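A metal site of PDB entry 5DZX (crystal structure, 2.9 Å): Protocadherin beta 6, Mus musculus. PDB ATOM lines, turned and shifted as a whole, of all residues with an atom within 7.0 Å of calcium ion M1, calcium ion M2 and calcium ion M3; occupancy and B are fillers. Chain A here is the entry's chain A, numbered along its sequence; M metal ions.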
ATOM      1  N   GLU A 225       8.479 -24.639 -31.876  1.00  0.00           N
ATOM      2  CA  GLU A 225       8.865 -23.284 -31.507  1.00  0.00           C
ATOM      3  C   GLU A 225      10.045 -23.264 -30.536  1.00  0.00           C
ATOM      4  O   GLU A 225      10.583 -22.206 -30.208  1.00  0.00           O
ATOM      5  CB  GLU A 225       7.680 -22.537 -30.884  1.00  0.00           C
ATOM      6  CG  GLU A 225       7.166 -23.150 -29.591  1.00  0.00           C
ATOM      7  CD  GLU A 225       6.138 -22.274 -28.902  1.00  0.00           C
ATOM      8  OE1 GLU A 225       5.616 -22.694 -27.852  1.00  0.00           O
ATOM      9  OE2 GLU A 225       5.854 -21.167 -29.404  1.00  0.00           O
ATOM     10  N   LEU A 278      12.081 -19.303 -31.795  1.00  0.00           N
ATOM     11  CA  LEU A 278      10.738 -19.175 -32.356  1.00  0.00           C
ATOM     12  C   LEU A 278       9.668 -19.102 -31.269  1.00  0.00           C
ATOM     13  O   LEU A 278       9.954 -19.334 -30.092  1.00  0.00           O
ATOM     14  CB  LEU A 278      10.426 -20.327 -33.289  1.00  0.00           C
ATOM     15  CG  LEU A 278      11.161 -20.339 -34.629  1.00  0.00           C
ATOM     16  CD1 LEU A 278      10.810 -21.583 -35.413  1.00  0.00           C
ATOM     17  CD2 LEU A 278      10.795 -19.090 -35.408  1.00  0.00           C
ATOM     18  N   ASP A 279       8.454 -18.781 -31.684  1.00  0.00           N
ATOM     19  CA  ASP A 279       7.317 -18.721 -30.784  1.00  0.00           C
ATOM     20  C   ASP A 279       6.009 -18.801 -31.562  1.00  0.00           C
ATOM     21  O   ASP A 279       5.755 -17.975 -32.441  1.00  0.00           O
ATOM     22  CB  ASP A 279       7.354 -17.449 -29.937  1.00  0.00           C
ATOM     23  CG  ASP A 279       6.326 -17.463 -28.828  1.00  0.00           C
ATOM     24  OD1 ASP A 279       6.664 -17.904 -27.711  1.00  0.00           O
ATOM     25  OD2 ASP A 279       5.167 -17.041 -29.067  1.00  0.00           O
ATOM     26  N   PHE A 280       5.192 -19.801 -31.237  1.00  0.00           N
ATOM     27  CA  PHE A 280       3.934 -20.032 -31.934  1.00  0.00           C
ATOM     28  C   PHE A 280       2.933 -18.924 -31.627  1.00  0.00           C
ATOM     29  O   PHE A 280       2.089 -18.587 -32.463  1.00  0.00           O
ATOM     30  CB  PHE A 280       3.355 -21.391 -31.539  1.00  0.00           C
ATOM     31  CG  PHE A 280       2.185 -21.823 -32.384  1.00  0.00           C
ATOM     32  CD1 PHE A 280       0.893 -21.466 -32.056  1.00  0.00           C
ATOM     33  CD2 PHE A 280       2.383 -22.619 -33.505  1.00  0.00           C
ATOM     34  CE1 PHE A 280      -0.184 -21.868 -32.836  1.00  0.00           C
ATOM     35  CE2 PHE A 280       1.305 -23.021 -34.285  1.00  0.00           C
ATOM     36  CZ  PHE A 280       0.026 -22.647 -33.947  1.00  0.00           C
ATOM     37  N   GLU A 281       3.015 -18.363 -30.428  1.00  0.00           N
ATOM     38  CA  GLU A 281       2.092 -17.325 -30.003  1.00  0.00           C
ATOM     39  C   GLU A 281       2.336 -16.022 -30.755  1.00  0.00           C
ATOM     40  O   GLU A 281       1.414 -15.229 -30.980  1.00  0.00           O
ATOM     41  CB  GLU A 281       2.177 -17.095 -28.488  1.00  0.00           C
ATOM     42  CG  GLU A 281       1.623 -18.233 -27.631  1.00  0.00           C
ATOM     43  CD  GLU A 281       2.509 -19.466 -27.629  1.00  0.00           C
ATOM     44  OE1 GLU A 281       3.719 -19.337 -27.897  1.00  0.00           O
ATOM     45  OE2 GLU A 281       1.993 -20.567 -27.353  1.00  0.00           O
ATOM     46  N   ALA A 282       3.581 -15.794 -31.150  1.00  0.00           N
ATOM     47  CA  ALA A 282       3.939 -14.582 -31.885  1.00  0.00           C
ATOM     48  C   ALA A 282       3.656 -14.731 -33.370  1.00  0.00           C
ATOM     49  O   ALA A 282       2.817 -14.030 -33.930  1.00  0.00           O
ATOM     50  CB  ALA A 282       5.415 -14.240 -31.658  1.00  0.00           C
ATOM     51  N   LEU A 309       4.916 -25.451 -34.988  1.00  0.00           N
ATOM     52  CA  LEU A 309       4.014 -26.297 -34.214  1.00  0.00           C
ATOM     53  C   LEU A 309       3.945 -25.819 -32.776  1.00  0.00           C
ATOM     54  O   LEU A 309       4.972 -25.586 -32.142  1.00  0.00           O
ATOM     55  CB  LEU A 309       4.469 -27.754 -34.272  1.00  0.00           C
ATOM     56  CG  LEU A 309       4.570 -28.338 -35.683  1.00  0.00           C
ATOM     57  CD1 LEU A 309       5.054 -29.780 -35.639  1.00  0.00           C
ATOM     58  CD2 LEU A 309       3.232 -28.246 -36.396  1.00  0.00           C
ATOM     59  N   ASP A 310       2.728 -25.657 -32.268  1.00  0.00           N
ATOM     60  CA  ASP A 310       2.524 -25.153 -30.916  1.00  0.00           C
ATOM     61  C   ASP A 310       2.887 -26.183 -29.855  1.00  0.00           C
ATOM     62  O   ASP A 310       2.311 -27.270 -29.810  1.00  0.00           O
ATOM     63  CB  ASP A 310       1.085 -24.708 -30.713  1.00  0.00           C
ATOM     64  CG  ASP A 310       0.795 -24.315 -29.276  1.00  0.00           C
ATOM     65  OD1 ASP A 310       1.033 -23.145 -28.912  1.00  0.00           O
ATOM     66  OD2 ASP A 310       0.311 -25.172 -28.504  1.00  0.00           O
ATOM     67  N   VAL A 311       3.856 -25.839 -29.021  1.00  0.00           N
ATOM     68  CA  VAL A 311       4.219 -26.693 -27.895  1.00  0.00           C
ATOM     69  C   VAL A 311       3.640 -26.100 -26.622  1.00  0.00           C
ATOM     70  O   VAL A 311       3.733 -24.893 -26.393  1.00  0.00           O
ATOM     71  CB  VAL A 311       5.757 -26.837 -27.771  1.00  0.00           C
ATOM     72  CG1 VAL A 311       6.116 -27.686 -26.557  1.00  0.00           C
ATOM     73  CG2 VAL A 311       6.334 -27.440 -29.045  1.00  0.00           C
ATOM     74  N   ASN A 312       3.022 -26.937 -25.794  1.00  0.00           N
ATOM     75  CA  ASN A 312       2.390 -26.470 -24.564  1.00  0.00           C
ATOM     76  C   ASN A 312       3.449 -26.033 -23.552  1.00  0.00           C
ATOM     77  O   ASN A 312       3.705 -26.732 -22.568  1.00  0.00           O
ATOM     78  CB  ASN A 312       1.503 -27.566 -23.972  1.00  0.00           C
ATOM     79  CG  ASN A 312       0.637 -27.060 -22.834  1.00  0.00           C
ATOM     80  OD1 ASN A 312       0.290 -25.887 -22.776  1.00  0.00           O
ATOM     81  ND2 ASN A 312       0.286 -27.954 -21.912  1.00  0.00           N
ATOM     82  N   ASP A 313       4.058 -24.885 -23.804  1.00  0.00           N
ATOM     83  CA  ASP A 313       5.136 -24.367 -22.972  1.00  0.00           C
ATOM     84  C   ASP A 313       4.652 -23.366 -21.934  1.00  0.00           C
ATOM     85  O   ASP A 313       5.405 -22.972 -21.046  1.00  0.00           O
ATOM     86  CB  ASP A 313       6.192 -23.703 -23.851  1.00  0.00           C
ATOM     87  CG  ASP A 313       5.646 -22.516 -24.637  1.00  0.00           C
ATOM     88  OD1 ASP A 313       4.420 -22.485 -24.878  1.00  0.00           O
ATOM     89  OD2 ASP A 313       6.426 -21.606 -24.992  1.00  0.00           O
ATOM     90  N   ASN A 314       3.396 -22.943 -22.058  1.00  0.00           N
ATOM     91  CA  ASN A 314       2.836 -21.966 -21.136  1.00  0.00           C
ATOM     92  C   ASN A 314       1.730 -22.526 -20.246  1.00  0.00           C
ATOM     93  O   ASN A 314       0.742 -23.077 -20.730  1.00  0.00           O
ATOM     94  CB  ASN A 314       2.301 -20.762 -21.912  1.00  0.00           C
ATOM     95  CG  ASN A 314       3.376 -20.100 -22.749  1.00  0.00           C
ATOM     96  OD1 ASN A 314       3.204 -19.870 -23.949  1.00  0.00           O
ATOM     97  ND2 ASN A 314       4.506 -19.786 -22.121  1.00  0.00           N
ATOM     98  N   ALA A 315       1.898 -22.380 -18.935  1.00  0.00           N
ATOM     99  CA  ALA A 315       0.904 -22.853 -17.978  1.00  0.00           C
ATOM    100  C   ALA A 315      -0.225 -21.837 -17.803  1.00  0.00           C
ATOM    101  O   ALA A 315      -0.003 -20.626 -17.922  1.00  0.00           O
ATOM    102  CB  ALA A 315       1.566 -23.150 -16.630  1.00  0.00           C
ATOM    103  N   PRO A 316      -1.452 -22.325 -17.549  1.00  0.00           N
ATOM    104  CA  PRO A 316      -2.644 -21.520 -17.283  1.00  0.00           C
ATOM    105  C   PRO A 316      -2.395 -20.400 -16.272  1.00  0.00           C
ATOM    106  O   PRO A 316      -1.646 -20.590 -15.321  1.00  0.00           O
ATOM    107  CB  PRO A 316      -3.632 -22.541 -16.697  1.00  0.00           C
ATOM    108  CG  PRO A 316      -3.156 -23.885 -17.167  1.00  0.00           C
ATOM    109  CD  PRO A 316      -1.786 -23.751 -17.770  1.00  0.00           C
ATOM    110  N   ASP A 343      -4.939 -18.679 -21.135  1.00  0.00           N
ATOM    111  CA  ASP A 343      -3.891 -19.566 -21.625  1.00  0.00           C
ATOM    112  C   ASP A 343      -3.490 -19.154 -23.037  1.00  0.00           C
ATOM    113  O   ASP A 343      -4.297 -19.259 -23.957  1.00  0.00           O
ATOM    114  CB  ASP A 343      -4.357 -21.027 -21.605  1.00  0.00           C
ATOM    115  CG  ASP A 343      -3.203 -22.017 -21.668  1.00  0.00           C
ATOM    116  OD1 ASP A 343      -2.070 -21.616 -22.012  1.00  0.00           O
ATOM    117  OD2 ASP A 343      -3.434 -23.215 -21.387  1.00  0.00           O
ATOM    118  N   PRO A 344      -2.249 -18.674 -23.215  1.00  0.00           N
ATOM    119  CA  PRO A 344      -1.779 -18.166 -24.504  1.00  0.00           C
ATOM    120  C   PRO A 344      -1.589 -19.239 -25.579  1.00  0.00           C
ATOM    121  O   PRO A 344      -1.628 -18.926 -26.771  1.00  0.00           O
ATOM    122  CB  PRO A 344      -0.431 -17.527 -24.151  1.00  0.00           C
ATOM    123  CG  PRO A 344       0.023 -18.260 -22.949  1.00  0.00           C
ATOM    124  CD  PRO A 344      -1.221 -18.551 -22.162  1.00  0.00           C
ATOM    125  N   ASP A 345      -1.387 -20.489 -25.158  1.00  0.00           N
ATOM    126  CA  ASP A 345      -1.180 -21.593 -26.089  1.00  0.00           C
ATOM    127  C   ASP A 345      -2.384 -21.840 -26.988  1.00  0.00           C
ATOM    128  O   ASP A 345      -3.494 -21.393 -26.691  1.00  0.00           O
ATOM    129  CB  ASP A 345      -0.844 -22.874 -25.322  1.00  0.00           C
ATOM    130  CG  ASP A 345       0.467 -22.773 -24.554  1.00  0.00           C
ATOM    131  OD1 ASP A 345       1.421 -22.192 -25.089  1.00  0.00           O
ATOM    132  OD2 ASP A 345       0.512 -23.277 -23.408  1.00  0.00           O
ATOM    133  N   SER A 346      -2.166 -22.549 -28.093  1.00  0.00           N
ATOM    134  CA  SER A 346      -3.235 -22.848 -29.048  1.00  0.00           C
ATOM    135  C   SER A 346      -3.677 -24.310 -28.943  1.00  0.00           C
ATOM    136  O   SER A 346      -3.005 -25.121 -28.315  1.00  0.00           O
ATOM    137  CB  SER A 346      -2.776 -22.531 -30.476  1.00  0.00           C
ATOM    138  OG  SER A 346      -2.492 -21.151 -30.623  1.00  0.00           O
ATOM    139  N   ASP A 348      -5.614 -27.671 -27.838  1.00  0.00           N
ATOM    140  CA  ASP A 348      -6.015 -28.167 -26.529  1.00  0.00           C
ATOM    141  C   ASP A 348      -4.992 -27.793 -25.469  1.00  0.00           C
ATOM    142  O   ASP A 348      -5.172 -28.065 -24.290  1.00  0.00           O
ATOM    143  CB  ASP A 348      -6.216 -29.688 -26.562  1.00  0.00           C
ATOM    144  CG  ASP A 348      -7.426 -30.117 -27.374  1.00  0.00           C
ATOM    145  OD1 ASP A 348      -8.224 -29.240 -27.756  1.00  0.00           O
ATOM    146  OD2 ASP A 348      -7.573 -31.330 -27.622  1.00  0.00           O
ATOM    147  N   ASN A 349      -3.902 -27.168 -25.903  1.00  0.00           N
ATOM    148  CA  ASN A 349      -2.896 -26.660 -24.988  1.00  0.00           C
ATOM    149  C   ASN A 349      -3.384 -25.356 -24.345  1.00  0.00           C
ATOM    150  O   ASN A 349      -2.900 -24.952 -23.292  1.00  0.00           O
ATOM    151  CB  ASN A 349      -1.563 -26.434 -25.700  1.00  0.00           C
ATOM    152  CG  ASN A 349      -1.049 -27.682 -26.400  1.00  0.00           C
ATOM    153  OD1 ASN A 349      -1.191 -28.787 -25.889  1.00  0.00           O
ATOM    154  ND2 ASN A 349      -0.443 -27.500 -27.562  1.00  0.00           N
ATOM    155  N   GLY A 350      -4.349 -24.723 -24.996  1.00  0.00           N
ATOM    156  CA  GLY A 350      -4.902 -23.466 -24.524  1.00  0.00           C
ATOM    157  C   GLY A 350      -6.304 -23.596 -23.962  1.00  0.00           C
ATOM    158  O   GLY A 350      -6.900 -22.607 -23.511  1.00  0.00           O
ATOM    159  N   ARG A 351      -6.846 -24.804 -23.979  1.00  0.00           N
ATOM    160  CA  ARG A 351      -8.144 -25.079 -23.381  1.00  0.00           C
ATOM    161  C   ARG A 351      -7.930 -25.460 -21.925  1.00  0.00           C
ATOM    162  O   ARG A 351      -7.089 -26.304 -21.611  1.00  0.00           O
ATOM    163  CB  ARG A 351      -8.883 -26.193 -24.111  1.00  0.00           C
ATOM    164  CG  ARG A 351      -9.397 -25.830 -25.492  1.00  0.00           C
ATOM    165  CD  ARG A 351      -9.980 -27.047 -26.195  1.00  0.00           C
ATOM    166  NE  ARG A 351     -11.094 -27.630 -25.455  1.00  0.00           N
ATOM    167  CZ  ARG A 351     -11.679 -28.783 -25.769  1.00  0.00           C
ATOM    168  NH1 ARG A 351     -12.695 -29.240 -25.039  1.00  0.00           N
ATOM    169  NH2 ARG A 351     -11.262 -29.476 -26.813  1.00  0.00           N
ATOM    170  N   MET A 352      -8.692 -24.850 -21.027  1.00  0.00           N
ATOM    171  CA  MET A 352      -8.490 -25.055 -19.607  1.00  0.00           C
ATOM    172  C   MET A 352      -9.730 -25.589 -18.920  1.00  0.00           C
ATOM    173  O   MET A 352     -10.864 -25.280 -19.307  1.00  0.00           O
ATOM    174  CB  MET A 352      -8.053 -23.758 -18.935  1.00  0.00           C
ATOM    175  CG  MET A 352      -6.730 -23.207 -19.422  1.00  0.00           C
ATOM    176  SD  MET A 352      -6.507 -21.486 -18.917  1.00  0.00           S
ATOM    177  CE  MET A 352      -7.769 -20.690 -19.920  1.00  0.00           C
ATOM    178  N   ASP A 396      -4.671 -27.146 -18.016  1.00  0.00           N
ATOM    179  CA  ASP A 396      -4.976 -27.231 -19.429  1.00  0.00           C
ATOM    180  C   ASP A 396      -5.129 -28.689 -19.864  1.00  0.00           C
ATOM    181  O   ASP A 396      -4.832 -29.598 -19.091  1.00  0.00           O
ATOM    182  CB  ASP A 396      -3.902 -26.537 -20.267  1.00  0.00           C
ATOM    183  CG  ASP A 396      -2.494 -26.988 -19.899  1.00  0.00           C
ATOM    184  OD1 ASP A 396      -2.351 -28.047 -19.254  1.00  0.00           O
ATOM    185  OD2 ASP A 396      -1.536 -26.289 -20.287  1.00  0.00           O
ATOM    186  N   LEU A 397      -5.548 -28.896 -21.098  1.00  0.00           N
ATOM    187  CA  LEU A 397      -5.741 -30.243 -21.631  1.00  0.00           C
ATOM    188  C   LEU A 397      -4.642 -30.625 -22.601  1.00  0.00           C
ATOM    189  O   LEU A 397      -4.828 -31.485 -23.470  1.00  0.00           O
ATOM    190  CB  LEU A 397      -7.115 -30.347 -22.309  1.00  0.00           C
ATOM    191  CG  LEU A 397      -8.303 -30.004 -21.413  1.00  0.00           C
ATOM    192  CD1 LEU A 397      -9.597 -29.998 -22.218  1.00  0.00           C
ATOM    193  CD2 LEU A 397      -8.394 -30.990 -20.260  1.00  0.00           C
ATOM    194  N   GLY A 398      -3.477 -29.990 -22.452  1.00  0.00           N
ATOM    195  CA  GLY A 398      -2.363 -30.233 -23.345  1.00  0.00           C
ATOM    196  C   GLY A 398      -1.537 -31.456 -22.991  1.00  0.00           C
ATOM    197  O   GLY A 398      -1.868 -32.191 -22.053  1.00  0.00           O
ATOM    198  N   PRO A 400       2.488 -32.359 -22.208  1.00  0.00           N
ATOM    199  CA  PRO A 400       1.852 -32.771 -20.953  1.00  0.00           C
ATOM    200  C   PRO A 400       0.899 -31.709 -20.398  1.00  0.00           C
ATOM    201  O   PRO A 400       0.786 -30.635 -20.991  1.00  0.00           O
ATOM    202  CB  PRO A 400       3.045 -32.959 -19.996  1.00  0.00           C
ATOM    203  CG  PRO A 400       4.257 -33.017 -20.887  1.00  0.00           C
ATOM    204  CD  PRO A 400       3.926 -32.134 -22.038  1.00  0.00           C
ATOM    205  N   LEU A 402      -0.245 -28.852 -17.885  1.00  0.00           N
ATOM    206  CA  LEU A 402       0.317 -27.843 -16.991  1.00  0.00           C
ATOM    207  C   LEU A 402      -0.741 -27.337 -16.013  1.00  0.00           C
ATOM    208  O   LEU A 402      -1.875 -27.057 -16.413  1.00  0.00           O
ATOM    209  CB  LEU A 402       0.905 -26.684 -17.781  1.00  0.00           C
ATOM    210  CG  LEU A 402       2.038 -27.043 -18.749  1.00  0.00           C
ATOM    211  CD1 LEU A 402       2.411 -25.862 -19.614  1.00  0.00           C
ATOM    212  CD2 LEU A 402       3.240 -27.571 -17.991  1.00  0.00           C
HETATM  213 CA    CA M   1       5.771 -19.979 -26.665  1.00  0.00          CA
HETATM  214 CA    CA M   2       3.184 -22.723 -27.132  1.00  0.00          CA
HETATM  215 CA    CA M   3      -1.074 -24.162 -21.980  1.00  0.00          CA
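The backbone carbonyl oxygen (O) of Pro 400 is in hydrogen-bond range of the side-chain amide nitrogen (ND2) of Asn 312 (2.9 Å). The side-chain amide nitrogen of Asn 349 is in hydrogen-bond range of the side-chain carboxylate of Asp 310, at 2.6 Å. OD1 of Asp 313 lies close to OD1 of Asn 314 (3.0 Å). The backbone NH of Ala 282 sits at hydrogen-bond distance from the side-chain carboxylate of Asp 279, 2.9 Å away. OD1 of Asp 396 sits at hydrogen-bond distance from N of Leu 402, at 2.6 Å. The side-chain carboxylate (OD1) of Asp 310 sits close to the backbone NH (N) of Ser 346 (3.4 Å).
Calcium ion M2 is bound by O of Val 311 (2.4 Å), OE2 of Glu 281 (2.5 Å), OE1 of Glu 225 (2.5 Å), OD1 of Asp 313 (2.6 Å), OD1 of Asp 345 (2.8 Å) and OD1 of Asp 310 (2.8 Å).
The side-chain carboxylate (OD2) of Asp 313 is bound to calcium ion M1 (2.4 Å). The side-chain carboxylate (OE1) of Glu 281 binds calcium ion M1. OD1 of Asp 279 is bound to calcium ion M1 (2.5 Å). Calcium ion M1 has three donor atoms within binding distance. Slightly farther from calcium ion M1 lies the side-chain carboxylate (OE1) of Glu 225 (3.0 Å). Slightly farther from calcium ion M1 lies OE2 of Glu 225 (3.0 Å).
Within 4 Å of calcium ion M3: Asn 312, Asn 314, Asp 343, Asp 345, Asn 349 and Asp 396.
Of the 28 residues printed, 6 come within 4 Å of calcium ion M2. The nearest printed residue that does not touch calcium ion M2 is Asn 314 (4.3 Å).
Five residues have an atom within 4 Å of calcium ion M1: Glu 225, Asp 279, Glu 281, Asp 313 and Asn 314. Along chain A the residues within 4 Å of calcium ion M1 span positions 225 to 314. The nearest printed residue that does not touch calcium ion M1 is Phe 280 (4.6 Å).
Calcium ion M3 is bound by OD2 of Asp 345 (2.3 Å), OD1 of Asn 312 (2.3 Å), O of Asn 349 (2.4 Å), O of Asn 314 (2.5 Å), OD2 of Asp 343 (2.6 Å), OD1 of Asp 343 (2.7 Å) and OD2 of Asp 396 (2.8 Å). Calcium ion M3 has seven donor atoms within binding distance.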
